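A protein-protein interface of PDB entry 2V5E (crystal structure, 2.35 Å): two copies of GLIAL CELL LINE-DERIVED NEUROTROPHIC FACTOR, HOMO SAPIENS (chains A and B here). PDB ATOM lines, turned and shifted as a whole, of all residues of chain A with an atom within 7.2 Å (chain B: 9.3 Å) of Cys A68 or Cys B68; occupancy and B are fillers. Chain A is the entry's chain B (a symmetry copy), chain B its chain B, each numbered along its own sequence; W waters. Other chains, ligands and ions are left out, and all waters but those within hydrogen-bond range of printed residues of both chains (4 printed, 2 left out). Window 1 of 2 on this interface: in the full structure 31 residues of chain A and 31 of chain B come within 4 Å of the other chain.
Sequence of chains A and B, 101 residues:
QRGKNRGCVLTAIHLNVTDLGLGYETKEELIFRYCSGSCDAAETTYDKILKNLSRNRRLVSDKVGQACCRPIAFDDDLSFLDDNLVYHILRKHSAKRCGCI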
ATOM      1  N   CYS A   8      -4.158 -18.982  18.079  1.00  0.00           N
ATOM      2  CA  CYS A   8      -5.333 -19.206  18.922  1.00  0.00           C
ATOM      3  C   CYS A   8      -4.796 -19.890  20.176  1.00  0.00           C
ATOM      4  O   CYS A   8      -4.383 -21.048  20.123  1.00  0.00           O
ATOM      5  CB  CYS A   8      -6.361 -20.077  18.174  1.00  0.00           C
ATOM      6  SG  CYS A   8      -7.822 -20.654  19.089  1.00  0.00           S
ATOM      7  N   CYS A  35      -9.628 -18.256  25.818  1.00  0.00           N
ATOM      8  CA  CYS A  35      -9.092 -18.553  24.497  1.00  0.00           C
ATOM      9  C   CYS A  35      -9.197 -17.318  23.625  1.00  0.00           C
ATOM     10  O   CYS A  35     -10.285 -16.770  23.489  1.00  0.00           O
ATOM     11  CB  CYS A  35      -9.902 -19.680  23.861  1.00  0.00           C
ATOM     12  SG  CYS A  35      -9.657 -21.300  24.641  1.00  0.00           S
ATOM     13  N   GLY A  37      -7.194 -15.112  19.930  1.00  0.00           N
ATOM     14  CA  GLY A  37      -6.285 -15.125  18.785  1.00  0.00           C
ATOM     15  C   GLY A  37      -7.033 -15.375  17.484  1.00  0.00           C
ATOM     16  O   GLY A  37      -8.228 -15.701  17.486  1.00  0.00           O
ATOM     17  N   SER A  38      -6.329 -15.237  16.369  1.00  0.00           N
ATOM     18  CA  SER A  38      -6.981 -15.245  15.058  1.00  0.00           C
ATOM     19  C   SER A  38      -7.244 -16.651  14.501  1.00  0.00           C
ATOM     20  O   SER A  38      -6.530 -17.613  14.809  1.00  0.00           O
ATOM     21  CB  SER A  38      -6.162 -14.418  14.068  1.00  0.00           C
ATOM     22  OG  SER A  38      -4.987 -15.116  13.755  1.00  0.00           O
ATOM     23  N   CYS A  39      -8.295 -16.740  13.693  1.00  0.00           N
ATOM     24  CA  CYS A  39      -8.708 -17.964  13.009  1.00  0.00           C
ATOM     25  C   CYS A  39      -8.886 -17.697  11.513  1.00  0.00           C
ATOM     26  O   CYS A  39      -9.927 -18.019  10.918  1.00  0.00           O
ATOM     27  CB  CYS A  39     -10.015 -18.487  13.614  1.00  0.00           C
ATOM     28  SG  CYS A  39      -9.790 -19.029  15.295  1.00  0.00           S
ATOM     29  N   ASP A  47     -15.502 -23.529   6.024  1.00  0.00           N
ATOM     30  CA  ASP A  47     -14.599 -22.392   6.180  1.00  0.00           C
ATOM     31  C   ASP A  47     -13.798 -22.129   4.904  1.00  0.00           C
ATOM     32  O   ASP A  47     -13.528 -20.965   4.565  1.00  0.00           O
ATOM     33  CB  ASP A  47     -13.666 -22.612   7.379  1.00  0.00           C
ATOM     34  CG  ASP A  47     -14.417 -22.591   8.733  1.00  0.00           C
ATOM     35  OD1 ASP A  47     -15.297 -21.725   8.938  1.00  0.00           O
ATOM     36  OD2 ASP A  47     -14.120 -23.431   9.603  1.00  0.00           O
ATOM     37  N   GLY A  65     -18.822 -14.446   8.701  1.00  0.00           N
ATOM     38  CA  GLY A  65     -19.119 -15.800   9.199  1.00  0.00           C
ATOM     39  C   GLY A  65     -17.899 -16.608   9.620  1.00  0.00           C
ATOM     40  O   GLY A  65     -17.955 -17.839   9.755  1.00  0.00           O
ATOM     41  N   GLN A  66     -16.795 -15.906   9.852  1.00  0.00           N
ATOM     42  CA  GLN A  66     -15.517 -16.537  10.142  1.00  0.00           C
ATOM     43  C   GLN A  66     -15.558 -17.325  11.449  1.00  0.00           C
ATOM     44  O   GLN A  66     -16.330 -17.005  12.358  1.00  0.00           O
ATOM     45  CB  GLN A  66     -14.412 -15.470  10.188  1.00  0.00           C
ATOM     46  CG  GLN A  66     -13.001 -15.989   9.933  1.00  0.00           C
ATOM     47  CD  GLN A  66     -12.005 -14.870   9.589  1.00  0.00           C
ATOM     48  OE1 GLN A  66     -11.925 -13.850  10.283  1.00  0.00           O
ATOM     49  NE2 GLN A  66     -11.237 -15.072   8.519  1.00  0.00           N
ATOM     50  N   ALA A  67     -14.728 -18.363  11.518  1.00  0.00           N
ATOM     51  CA  ALA A  67     -14.477 -19.091  12.750  1.00  0.00           C
ATOM     52  C   ALA A  67     -13.858 -18.177  13.811  1.00  0.00           C
ATOM     53  O   ALA A  67     -13.326 -17.131  13.479  1.00  0.00           O
ATOM     54  CB  ALA A  67     -13.563 -20.292  12.463  1.00  0.00           C
ATOM     55  N   CYS A  68     -13.931 -18.569  15.081  1.00  0.00           N
ATOM     56  CA  CYS A  68     -13.261 -17.823  16.168  1.00  0.00           C
ATOM     57  C   CYS A  68     -12.594 -18.733  17.203  1.00  0.00           C
ATOM     58  O   CYS A  68     -12.937 -19.899  17.330  1.00  0.00           O
ATOM     59  CB  CYS A  68     -14.212 -16.834  16.858  1.00  0.00           C
ATOM     60  SG  CYS A  68     -15.689 -17.627  17.588  1.00  0.00           S
ATOM     61  N   CYS A  69     -11.633 -18.176  17.933  1.00  0.00           N
ATOM     62  CA  CYS A  69     -10.841 -18.919  18.901  1.00  0.00           C
ATOM     63  C   CYS A  69     -11.603 -19.118  20.229  1.00  0.00           C
ATOM     64  O   CYS A  69     -11.845 -18.160  20.977  1.00  0.00           O
ATOM     65  CB  CYS A  69      -9.532 -18.181  19.125  1.00  0.00           C
ATOM     66  SG  CYS A  69      -8.394 -19.036  20.181  1.00  0.00           S
ATOM     67  N   ARG A  70     -11.967 -20.367  20.506  1.00  0.00           N
ATOM     68  CA  ARG A  70     -12.945 -20.690  21.535  1.00  0.00           C
ATOM     69  C   ARG A  70     -12.529 -21.932  22.327  1.00  0.00           C
ATOM     70  O   ARG A  70     -11.710 -22.724  21.852  1.00  0.00           O
ATOM     71  CB  ARG A  70     -14.315 -20.918  20.879  1.00  0.00           C
ATOM     72  CG  ARG A  70     -14.945 -19.658  20.245  1.00  0.00           C
ATOM     73  CD  ARG A  70     -15.381 -18.612  21.300  1.00  0.00           C
ATOM     74  NE  ARG A  70     -16.567 -19.062  22.027  1.00  0.00           N
ATOM     75  CZ  ARG A  70     -17.085 -18.467  23.101  1.00  0.00           C
ATOM     76  NH1 ARG A  70     -16.523 -17.368  23.626  1.00  0.00           N
ATOM     77  NH2 ARG A  70     -18.170 -18.991  23.662  1.00  0.00           N
ATOM     78  N   PRO A  71     -13.076 -22.109  23.549  1.00  0.00           N
ATOM     79  CA  PRO A  71     -12.684 -23.308  24.297  1.00  0.00           C
ATOM     80  C   PRO A  71     -13.217 -24.555  23.616  1.00  0.00           C
ATOM     81  O   PRO A  71     -14.384 -24.570  23.191  1.00  0.00           O
ATOM     82  CB  PRO A  71     -13.380 -23.137  25.654  1.00  0.00           C
ATOM     83  CG  PRO A  71     -13.759 -21.698  25.725  1.00  0.00           C
ATOM     84  CD  PRO A  71     -13.984 -21.244  24.317  1.00  0.00           C
ATOM     85  N   GLY A  99      -9.459 -23.813  20.355  1.00  0.00           N
ATOM     86  CA  GLY A  99      -9.499 -24.118  18.935  1.00  0.00           C
ATOM     87  C   GLY A  99     -10.398 -23.143  18.208  1.00  0.00           C
ATOM     88  O   GLY A  99     -11.201 -22.439  18.832  1.00  0.00           O
ATOM     89  N   CYS A 100     -10.246 -23.109  16.887  1.00  0.00           N
ATOM     90  CA  CYS A 100     -11.092 -22.321  15.999  1.00  0.00           C
ATOM     91  C   CYS A 100     -12.329 -23.130  15.652  1.00  0.00           C
ATOM     92  O   CYS A 100     -12.214 -24.265  15.212  1.00  0.00           O
ATOM     93  CB  CYS A 100     -10.310 -21.954  14.731  1.00  0.00           C
ATOM     94  SG  CYS A 100      -8.910 -20.846  15.062  1.00  0.00           S
ATOM     95  N   ILE A 101     -13.508 -22.558  15.878  1.00  0.00           N
ATOM     96  CA  ILE A 101     -14.777 -23.273  15.686  1.00  0.00           C
ATOM     97  C   ILE A 101     -15.785 -22.333  15.052  1.00  0.00           C
ATOM     98  O   ILE A 101     -15.552 -21.109  15.056  1.00  0.00           O
ATOM     99  CB  ILE A 101     -15.369 -23.863  17.023  1.00  0.00           C
ATOM    100  CG1 ILE A 101     -15.693 -22.760  18.042  1.00  0.00           C
ATOM    101  CG2 ILE A 101     -14.440 -24.919  17.645  1.00  0.00           C
ATOM    102  CD1 ILE A 101     -16.285 -23.278  19.378  1.00  0.00           C
ATOM    103  OXT ILE A 101     -16.828 -22.767  14.530  1.00  0.00           O
ATOM    104  N   ASN B   5     -29.178 -12.661  20.941  1.00  0.00           N
ATOM    105  CA  ASN B   5     -28.442 -12.830  19.687  1.00  0.00           C
ATOM    106  C   ASN B   5     -29.332 -13.209  18.464  1.00  0.00           C
ATOM    107  O   ASN B   5     -28.956 -14.027  17.616  1.00  0.00           O
ATOM    108  CB  ASN B   5     -27.271 -13.812  19.891  1.00  0.00           C
ATOM    109  CG  ASN B   5     -26.322 -13.379  21.009  1.00  0.00           C
ATOM    110  OD1 ASN B   5     -25.899 -12.226  21.066  1.00  0.00           O
ATOM    111  ND2 ASN B   5     -25.955 -14.319  21.881  1.00  0.00           N
ATOM    112  N   CYS B   8     -27.987 -13.385  14.729  1.00  0.00           N
ATOM    113  CA  CYS B   8     -27.167 -14.479  14.208  1.00  0.00           C
ATOM    114  C   CYS B   8     -28.105 -15.289  13.318  1.00  0.00           C
ATOM    115  O   CYS B   8     -29.011 -15.958  13.817  1.00  0.00           O
ATOM    116  CB  CYS B   8     -26.598 -15.313  15.372  1.00  0.00           C
ATOM    117  SG  CYS B   8     -25.705 -16.845  14.970  1.00  0.00           S
ATOM    118  N   VAL B   9     -27.935 -15.173  11.999  1.00  0.00           N
ATOM    119  CA  VAL B   9     -28.930 -15.727  11.071  1.00  0.00           C
ATOM    120  C   VAL B   9     -28.344 -16.473   9.874  1.00  0.00           C
ATOM    121  O   VAL B   9     -27.154 -16.357   9.553  1.00  0.00           O
ATOM    122  CB  VAL B   9     -29.975 -14.642  10.582  1.00  0.00           C
ATOM    123  CG1 VAL B   9     -30.648 -13.918  11.774  1.00  0.00           C
ATOM    124  CG2 VAL B   9     -29.349 -13.641   9.643  1.00  0.00           C
ATOM    125  N   CYS B  35     -23.770 -18.765   8.125  1.00  0.00           N
ATOM    126  CA  CYS B  35     -24.225 -18.168   9.373  1.00  0.00           C
ATOM    127  C   CYS B  35     -23.445 -16.897   9.633  1.00  0.00           C
ATOM    128  O   CYS B  35     -22.220 -16.934   9.645  1.00  0.00           O
ATOM    129  CB  CYS B  35     -23.981 -19.144  10.522  1.00  0.00           C
ATOM    130  SG  CYS B  35     -25.055 -20.607  10.493  1.00  0.00           S
ATOM    131  N   SER B  36     -24.147 -15.781   9.849  1.00  0.00           N
ATOM    132  CA  SER B  36     -23.492 -14.509  10.197  1.00  0.00           C
ATOM    133  C   SER B  36     -24.362 -13.601  11.077  1.00  0.00           C
ATOM    134  O   SER B  36     -25.586 -13.751  11.127  1.00  0.00           O
ATOM    135  CB  SER B  36     -23.079 -13.758   8.939  1.00  0.00           C
ATOM    136  OG  SER B  36     -24.228 -13.224   8.324  1.00  0.00           O
ATOM    137  N   GLY B  37     -23.714 -12.659  11.757  1.00  0.00           N
ATOM    138  CA  GLY B  37     -24.380 -11.743  12.682  1.00  0.00           C
ATOM    139  C   GLY B  37     -23.696 -11.730  14.041  1.00  0.00           C
ATOM    140  O   GLY B  37     -22.809 -12.549  14.318  1.00  0.00           O
ATOM    141  N   SER B  38     -24.115 -10.809  14.897  1.00  0.00           N
ATOM    142  CA  SER B  38     -23.398 -10.560  16.149  1.00  0.00           C
ATOM    143  C   SER B  38     -23.773 -11.524  17.284  1.00  0.00           C
ATOM    144  O   SER B  38     -24.888 -12.055  17.340  1.00  0.00           O
ATOM    145  CB  SER B  38     -23.604  -9.110  16.585  1.00  0.00           C
ATOM    146  OG  SER B  38     -24.925  -8.951  17.029  1.00  0.00           O
ATOM    147  N   CYS B  39     -22.805 -11.743  18.168  1.00  0.00           N
ATOM    148  CA  CYS B  39     -22.947 -12.583  19.356  1.00  0.00           C
ATOM    149  C   CYS B  39     -22.491 -11.819  20.599  1.00  0.00           C
ATOM    150  O   CYS B  39     -21.668 -12.305  21.392  1.00  0.00           O
ATOM    151  CB  CYS B  39     -22.126 -13.867  19.191  1.00  0.00           C
ATOM    152  SG  CYS B  39     -22.775 -14.900  17.894  1.00  0.00           S
ATOM    153  N   ASP B  40     -23.036 -10.617  20.762  1.00  0.00           N
ATOM    154  CA  ASP B  40     -22.618  -9.728  21.836  1.00  0.00           C
ATOM    155  C   ASP B  40     -23.163 -10.148  23.192  1.00  0.00           C
ATOM    156  O   ASP B  40     -22.496  -9.971  24.195  1.00  0.00           O
ATOM    157  CB  ASP B  40     -23.037  -8.294  21.517  1.00  0.00           C
ATOM    158  CG  ASP B  40     -22.183  -7.663  20.433  1.00  0.00           C
ATOM    159  OD1 ASP B  40     -21.067  -8.165  20.180  1.00  0.00           O
ATOM    160  OD2 ASP B  40     -22.627  -6.646  19.849  1.00  0.00           O
ATOM    161  N   ALA B  41     -24.373 -10.699  23.212  1.00  0.00           N
ATOM    162  CA  ALA B  41     -25.017 -11.136  24.442  1.00  0.00           C
ATOM    163  C   ALA B  41     -24.470 -12.490  24.881  1.00  0.00           C
ATOM    164  O   ALA B  41     -24.367 -13.409  24.067  1.00  0.00           O
ATOM    165  CB  ALA B  41     -26.509 -11.216  24.248  1.00  0.00           C
ATOM    166  N   GLU B  43     -24.400 -16.069  26.541  1.00  0.00           N
ATOM    167  CA  GLU B  43     -25.355 -17.149  26.773  1.00  0.00           C
ATOM    168  C   GLU B  43     -24.758 -18.276  27.613  1.00  0.00           C
ATOM    169  O   GLU B  43     -25.437 -19.270  27.881  1.00  0.00           O
ATOM    170  CB  GLU B  43     -25.900 -17.713  25.449  1.00  0.00           C
ATOM    171  CG  GLU B  43     -26.324 -16.659  24.430  1.00  0.00           C
ATOM    172  CD  GLU B  43     -27.025 -17.244  23.211  1.00  0.00           C
ATOM    173  OE1 GLU B  43     -28.037 -17.949  23.395  1.00  0.00           O
ATOM    174  OE2 GLU B  43     -26.585 -16.975  22.072  1.00  0.00           O
ATOM    175  N   TYR B  46     -19.040 -19.012  30.829  1.00  0.00           N
ATOM    176  CA  TYR B  46     -17.737 -18.578  30.323  1.00  0.00           C
ATOM    177  C   TYR B  46     -17.829 -17.228  29.630  1.00  0.00           C
ATOM    178  O   TYR B  46     -16.984 -16.366  29.845  1.00  0.00           O
ATOM    179  CB  TYR B  46     -17.196 -19.629  29.351  1.00  0.00           C
ATOM    180  CG  TYR B  46     -15.937 -19.220  28.622  1.00  0.00           C
ATOM    181  CD1 TYR B  46     -14.689 -19.282  29.251  1.00  0.00           C
ATOM    182  CD2 TYR B  46     -15.993 -18.786  27.296  1.00  0.00           C
ATOM    183  CE1 TYR B  46     -13.516 -18.905  28.571  1.00  0.00           C
ATOM    184  CE2 TYR B  46     -14.832 -18.415  26.608  1.00  0.00           C
ATOM    185  CZ  TYR B  46     -13.600 -18.479  27.247  1.00  0.00           C
ATOM    186  OH  TYR B  46     -12.457 -18.123  26.556  1.00  0.00           O
ATOM    187  N   ASP B  47     -18.859 -17.072  28.792  1.00  0.00           N
ATOM    188  CA  ASP B  47     -19.124 -15.838  28.058  1.00  0.00           C
ATOM    189  C   ASP B  47     -19.549 -14.705  28.993  1.00  0.00           C
ATOM    190  O   ASP B  47     -19.192 -13.538  28.764  1.00  0.00           O
ATOM    191  CB  ASP B  47     -20.181 -16.079  26.971  1.00  0.00           C
ATOM    192  CG  ASP B  47     -19.674 -17.004  25.838  1.00  0.00           C
ATOM    193  OD1 ASP B  47     -18.518 -16.847  25.384  1.00  0.00           O
ATOM    194  OD2 ASP B  47     -20.433 -17.882  25.387  1.00  0.00           O
ATOM    195  N   LYS B  63     -14.366  -7.140  23.744  1.00  0.00           N
ATOM    196  CA  LYS B  63     -14.713  -8.169  22.745  1.00  0.00           C
ATOM    197  C   LYS B  63     -13.663  -9.296  22.541  1.00  0.00           C
ATOM    198  O   LYS B  63     -13.711 -10.039  21.554  1.00  0.00           O
ATOM    199  CB  LYS B  63     -15.122  -7.518  21.408  1.00  0.00           C
ATOM    200  N   VAL B  64     -12.741  -9.438  23.491  1.00  0.00           N
ATOM    201  CA  VAL B  64     -11.697 -10.468  23.412  1.00  0.00           C
ATOM    202  C   VAL B  64     -12.285 -11.859  23.712  1.00  0.00           C
ATOM    203  O   VAL B  64     -13.045 -12.018  24.679  1.00  0.00           O
ATOM    204  CB  VAL B  64     -10.485 -10.136  24.354  1.00  0.00           C
ATOM    205  CG1 VAL B  64     -10.825 -10.406  25.825  1.00  0.00           C
ATOM    206  CG2 VAL B  64      -9.231 -10.898  23.926  1.00  0.00           C
ATOM    207  N   GLY B  65     -11.955 -12.838  22.867  1.00  0.00           N
ATOM    208  CA  GLY B  65     -12.397 -14.233  23.040  1.00  0.00           C
ATOM    209  C   GLY B  65     -13.895 -14.454  22.869  1.00  0.00           C
ATOM    210  O   GLY B  65     -14.447 -15.483  23.286  1.00  0.00           O
ATOM    211  N   GLN B  66     -14.551 -13.491  22.232  1.00  0.00           N
ATOM    212  CA  GLN B  66     -15.998 -13.492  22.095  1.00  0.00           C
ATOM    213  C   GLN B  66     -16.489 -14.679  21.271  1.00  0.00           C
ATOM    214  O   GLN B  66     -15.770 -15.193  20.408  1.00  0.00           O
ATOM    215  CB  GLN B  66     -16.460 -12.168  21.466  1.00  0.00           C
ATOM    216  CG  GLN B  66     -17.908 -11.785  21.755  1.00  0.00           C
ATOM    217  CD  GLN B  66     -18.204 -10.305  21.465  1.00  0.00           C
ATOM    218  OE1 GLN B  66     -17.869  -9.784  20.395  1.00  0.00           O
ATOM    219  NE2 GLN B  66     -18.846  -9.633  22.420  1.00  0.00           N
ATOM    220  N   ALA B  67     -17.715 -15.110  21.559  1.00  0.00           N
ATOM    221  CA  ALA B  67     -18.422 -16.079  20.742  1.00  0.00           C
ATOM    222  C   ALA B  67     -18.651 -15.542  19.327  1.00  0.00           C
ATOM    223  O   ALA B  67     -18.579 -14.343  19.111  1.00  0.00           O
ATOM    224  CB  ALA B  67     -19.757 -16.442  21.410  1.00  0.00           C
ATOM    225  N   CYS B  68     -18.921 -16.424  18.368  1.00  0.00           N
ATOM    226  CA  CYS B  68     -19.276 -16.002  16.996  1.00  0.00           C
ATOM    227  C   CYS B  68     -20.411 -16.828  16.384  1.00  0.00           C
ATOM    228  O   CYS B  68     -20.681 -17.941  16.813  1.00  0.00           O
ATOM    229  CB  CYS B  68     -18.057 -15.993  16.063  1.00  0.00           C
ATOM    230  SG  CYS B  68     -17.231 -17.618  15.922  1.00  0.00           S
ATOM    231  N   CYS B  69     -21.069 -16.259  15.379  1.00  0.00           N
ATOM    232  CA  CYS B  69     -22.225 -16.869  14.742  1.00  0.00           C
ATOM    233  C   CYS B  69     -21.809 -17.957  13.727  1.00  0.00           C
ATOM    234  O   CYS B  69     -21.229 -17.660  12.673  1.00  0.00           O
ATOM    235  CB  CYS B  69     -23.041 -15.778  14.072  1.00  0.00           C
ATOM    236  SG  CYS B  69     -24.563 -16.348  13.363  1.00  0.00           S
ATOM    237  N   ARG B  70     -22.118 -19.207  14.060  1.00  0.00           N
ATOM    238  CA  ARG B  70     -21.538 -20.364  13.392  1.00  0.00           C
ATOM    239  C   ARG B  70     -22.583 -21.460  13.170  1.00  0.00           C
ATOM    240  O   ARG B  70     -23.619 -21.473  13.841  1.00  0.00           O
ATOM    241  CB  ARG B  70     -20.375 -20.907  14.236  1.00  0.00           C
ATOM    242  CG  ARG B  70     -19.153 -19.967  14.333  1.00  0.00           C
ATOM    243  CD  ARG B  70     -18.398 -19.827  12.989  1.00  0.00           C
ATOM    244  NE  ARG B  70     -17.662 -21.050  12.670  1.00  0.00           N
ATOM    245  CZ  ARG B  70     -17.053 -21.302  11.513  1.00  0.00           C
ATOM    246  NH1 ARG B  70     -17.080 -20.419  10.504  1.00  0.00           N
ATOM    247  NH2 ARG B  70     -16.420 -22.462  11.362  1.00  0.00           N
ATOM    248  N   PRO B  71     -22.332 -22.382  12.216  1.00  0.00           N
ATOM    249  CA  PRO B  71     -23.331 -23.438  12.018  1.00  0.00           C
ATOM    250  C   PRO B  71     -23.380 -24.354  13.227  1.00  0.00           C
ATOM    251  O   PRO B  71     -22.320 -24.737  13.748  1.00  0.00           O
ATOM    252  CB  PRO B  71     -22.799 -24.222  10.811  1.00  0.00           C
ATOM    253  CG  PRO B  71     -21.794 -23.329  10.171  1.00  0.00           C
ATOM    254  CD  PRO B  71     -21.218 -22.481  11.262  1.00  0.00           C
ATOM    255  N   ILE B  72     -24.590 -24.693  13.673  1.00  0.00           N
ATOM    256  CA  ILE B  72     -24.754 -25.708  14.720  1.00  0.00           C
ATOM    257  C   ILE B  72     -25.441 -26.953  14.150  1.00  0.00           C
ATOM    258  O   ILE B  72     -25.655 -27.939  14.859  1.00  0.00           O
ATOM    259  CB  ILE B  72     -25.463 -25.153  16.006  1.00  0.00           C
ATOM    260  CG1 ILE B  72     -26.855 -24.583  15.677  1.00  0.00           C
ATOM    261  CG2 ILE B  72     -24.561 -24.102  16.703  1.00  0.00           C
ATOM    262  CD1 ILE B  72     -27.745 -24.338  16.892  1.00  0.00           C
ATOM    263  N   CYS B  98     -28.035 -21.809  12.729  1.00  0.00           N
ATOM    264  CA  CYS B  98     -26.977 -20.963  13.257  1.00  0.00           C
ATOM    265  C   CYS B  98     -27.079 -20.785  14.754  1.00  0.00           C
ATOM    266  O   CYS B  98     -28.170 -20.839  15.324  1.00  0.00           O
ATOM    267  CB  CYS B  98     -26.995 -19.601  12.568  1.00  0.00           C
ATOM    268  SG  CYS B  98     -26.900 -19.798  10.783  1.00  0.00           S
ATOM    269  N   GLY B  99     -25.926 -20.592  15.390  1.00  0.00           N
ATOM    270  CA  GLY B  99     -25.871 -20.233  16.796  1.00  0.00           C
ATOM    271  C   GLY B  99     -24.539 -19.599  17.130  1.00  0.00           C
ATOM    272  O   GLY B  99     -23.577 -19.711  16.362  1.00  0.00           O
ATOM    273  N   CYS B 100     -24.503 -18.932  18.281  1.00  0.00           N
ATOM    274  CA  CYS B 100     -23.287 -18.347  18.834  1.00  0.00           C
ATOM    275  C   CYS B 100     -22.553 -19.407  19.637  1.00  0.00           C
ATOM    276  O   CYS B 100     -23.142 -20.032  20.506  1.00  0.00           O
ATOM    277  CB  CYS B 100     -23.648 -17.147  19.720  1.00  0.00           C
ATOM    278  SG  CYS B 100     -24.380 -15.775  18.784  1.00  0.00           S
ATOM    279  N   ILE B 101     -21.279 -19.626  19.325  1.00  0.00           N
ATOM    280  CA  ILE B 101     -20.490 -20.695  19.951  1.00  0.00           C
ATOM    281  C   ILE B 101     -19.090 -20.180  20.231  1.00  0.00           C
ATOM    282  O   ILE B 101     -18.712 -19.133  19.672  1.00  0.00           O
ATOM    283  CB  ILE B 101     -20.410 -22.005  19.078  1.00  0.00           C
ATOM    284  CG1 ILE B 101     -19.721 -21.752  17.728  1.00  0.00           C
ATOM    285  CG2 ILE B 101     -21.793 -22.641  18.869  1.00  0.00           C
ATOM    286  CD1 ILE B 101     -19.606 -23.007  16.825  1.00  0.00           C
ATOM    287  OXT ILE B 101     -18.327 -20.783  21.006  1.00  0.00           O
HETATM  288  O   HOH W   1     -19.182 -15.918  12.594  1.00  0.00           O
HETATM  289  O   HOH W   2     -10.063 -13.661  20.200  1.00  0.00           O
HETATM  290  O   HOH W   3     -12.793 -15.817  20.060  1.00  0.00           O
HETATM  291  O   HOH W   4     -20.554 -13.027  11.223  1.00  0.00           O
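The side-chain hydroxyl of Tyr B46 is in hydrogen-bond range of the backbone NH of Cys A35, 2.9 Å away.
OD1 of Asp B47 is in salt-bridge range of NH1 of Arg A70, 2.7 Å away.
NH1 of Arg A70 is in hydrogen-bond range of O of Gly B65 (2.8 Å).
SG of Cys A68 forms a disulfide with SG of Cys B68, 2.3 Å away.
The guanidinium group of Arg B70 lies within salt-bridge range of the side-chain carboxylate of Asp A47, 2.7 Å away.
The backbone carbonyl oxygen of Gly A65 lies within hydrogen-bond range of the guanidinium group of Arg B70.
The guanidinium group (NE) of Arg B70 is in salt-bridge range of the chain-end carboxylate (OXT) of Ile A101 (2.7 Å).
The guanidinium group (NE) of Arg A70 is in salt-bridge range of the chain-end carboxylate (OXT) of Ile B101, at 2.7 Å.
The backbone carbonyl oxygen (O) of Gln A66 lies close to the side-chain sulfur (SG) of Cys B68.
The backbone NH (N) of Ala A67 sits close to the guanidinium group (NH1) of Arg B70 (3.3 Å).
SG of Cys A68 lies close to O of Gln B66, 3.7 Å away.
NH1 of Arg A70 lies close to N of Ala B67 (3.3 Å).
The chain-end carboxylate (O) of Ile B101 is in hydrogen-bond range of the backbone NH (N) of Cys B68 (3.0 Å).
N of Arg B70 is in hydrogen-bond range of O of Gly B99 (2.8 Å).
The backbone NH (N) of Cys A68 lies within hydrogen-bond range of the chain-end carboxylate (O) of Ile A101 (3.0 Å).
O of Gly A99 lies within hydrogen-bond range of N of Arg A70 (2.8 Å).
SG of Cys B8 is disulfide-bonded to SG of Cys B69, at 2.0 Å.
SG of Cys B39 is disulfide-bonded to SG of Cys B100, 2.0 Å away.
Among the printed residues, merely in contact across the chains: Cys A35 with Gly B65 (3.3 Å), Gly A65 with Cys B35 (3.3 Å), Arg A70 with Gln B66 (3.6 Å), Gln A66 with Arg B70 (3.6 Å), Pro A71 with Tyr B46 (3.6 Å), Arg A70 with Tyr B46 (3.6 Å), Ile A101 with Ile B101 (3.6 Å), Cys A68 with Ile B101 (3.97 Å) and Ile A101 with Cys B68 (3.97 Å).
Printed residues of chain A within 4 Å of Cys B68: Gln A66 (3.7 Å), Cys A68 (2.3 Å) and Ile A101 (3.97 Å).
Cys A100 touches none of the printed residues of chain B.
Printed residues of chain B within 4 Å of Ala A67: Arg B70.
Of the printed residues of chain A, Cys B35 touches Gly A65 (3.3 Å).
Printed residues of chain B within 4 Å of Gly A65: Cys B35 (3.3 Å) and Arg B70 (2.8 Å).
Of the printed residues of chain A, Ala B67 touches Arg A70.
Printed residues of chain A within 4 Å of Tyr B46: Cys A35, Arg A70 and Pro A71.
Cys B69 touches none of the printed residues of chain A.
Of the 27 printed residues of chain B, 9 touch a printed residue of chain A.
Along chain B the printed residues that touch a printed residue of chain A span positions 35 to 101.
Hydrophobic or aromatic side chains of chain A within 4 Å of the printed part of chain B: Ala A67, Pro A71 and Ile A101.
Among the printed residues, 21 pairs touch across the chains.
Gly A65 touches Arg B70, and with the chains exchanged Arg A70 touches Gly B65.
Gln A66 touches Arg B70, and with the chains exchanged Arg A70 touches Gln B66.
Cys A68 touches Ile B101, and with the chains exchanged Ile A101 touches Cys B68.
Ile A101 touches its own counterpart, Ile B101.
Water W1 lies within hydrogen-bond range of O of Cys B69 (2.7 Å) and O of Gln A66 (3.1 Å).
Water W3 bridges O of Cys A69 (2.7 Å) and O of Gln B66 (3.1 Å).
Water W4 lies within hydrogen-bond range of N of Gly B37 (3.2 Å) and N of Gly A65 (3.4 Å).
Water W2 bridges the backbone NH (N) of Gly A37 (3.2 Å) and the backbone NH (N) of Gly B65 (3.4 Å).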
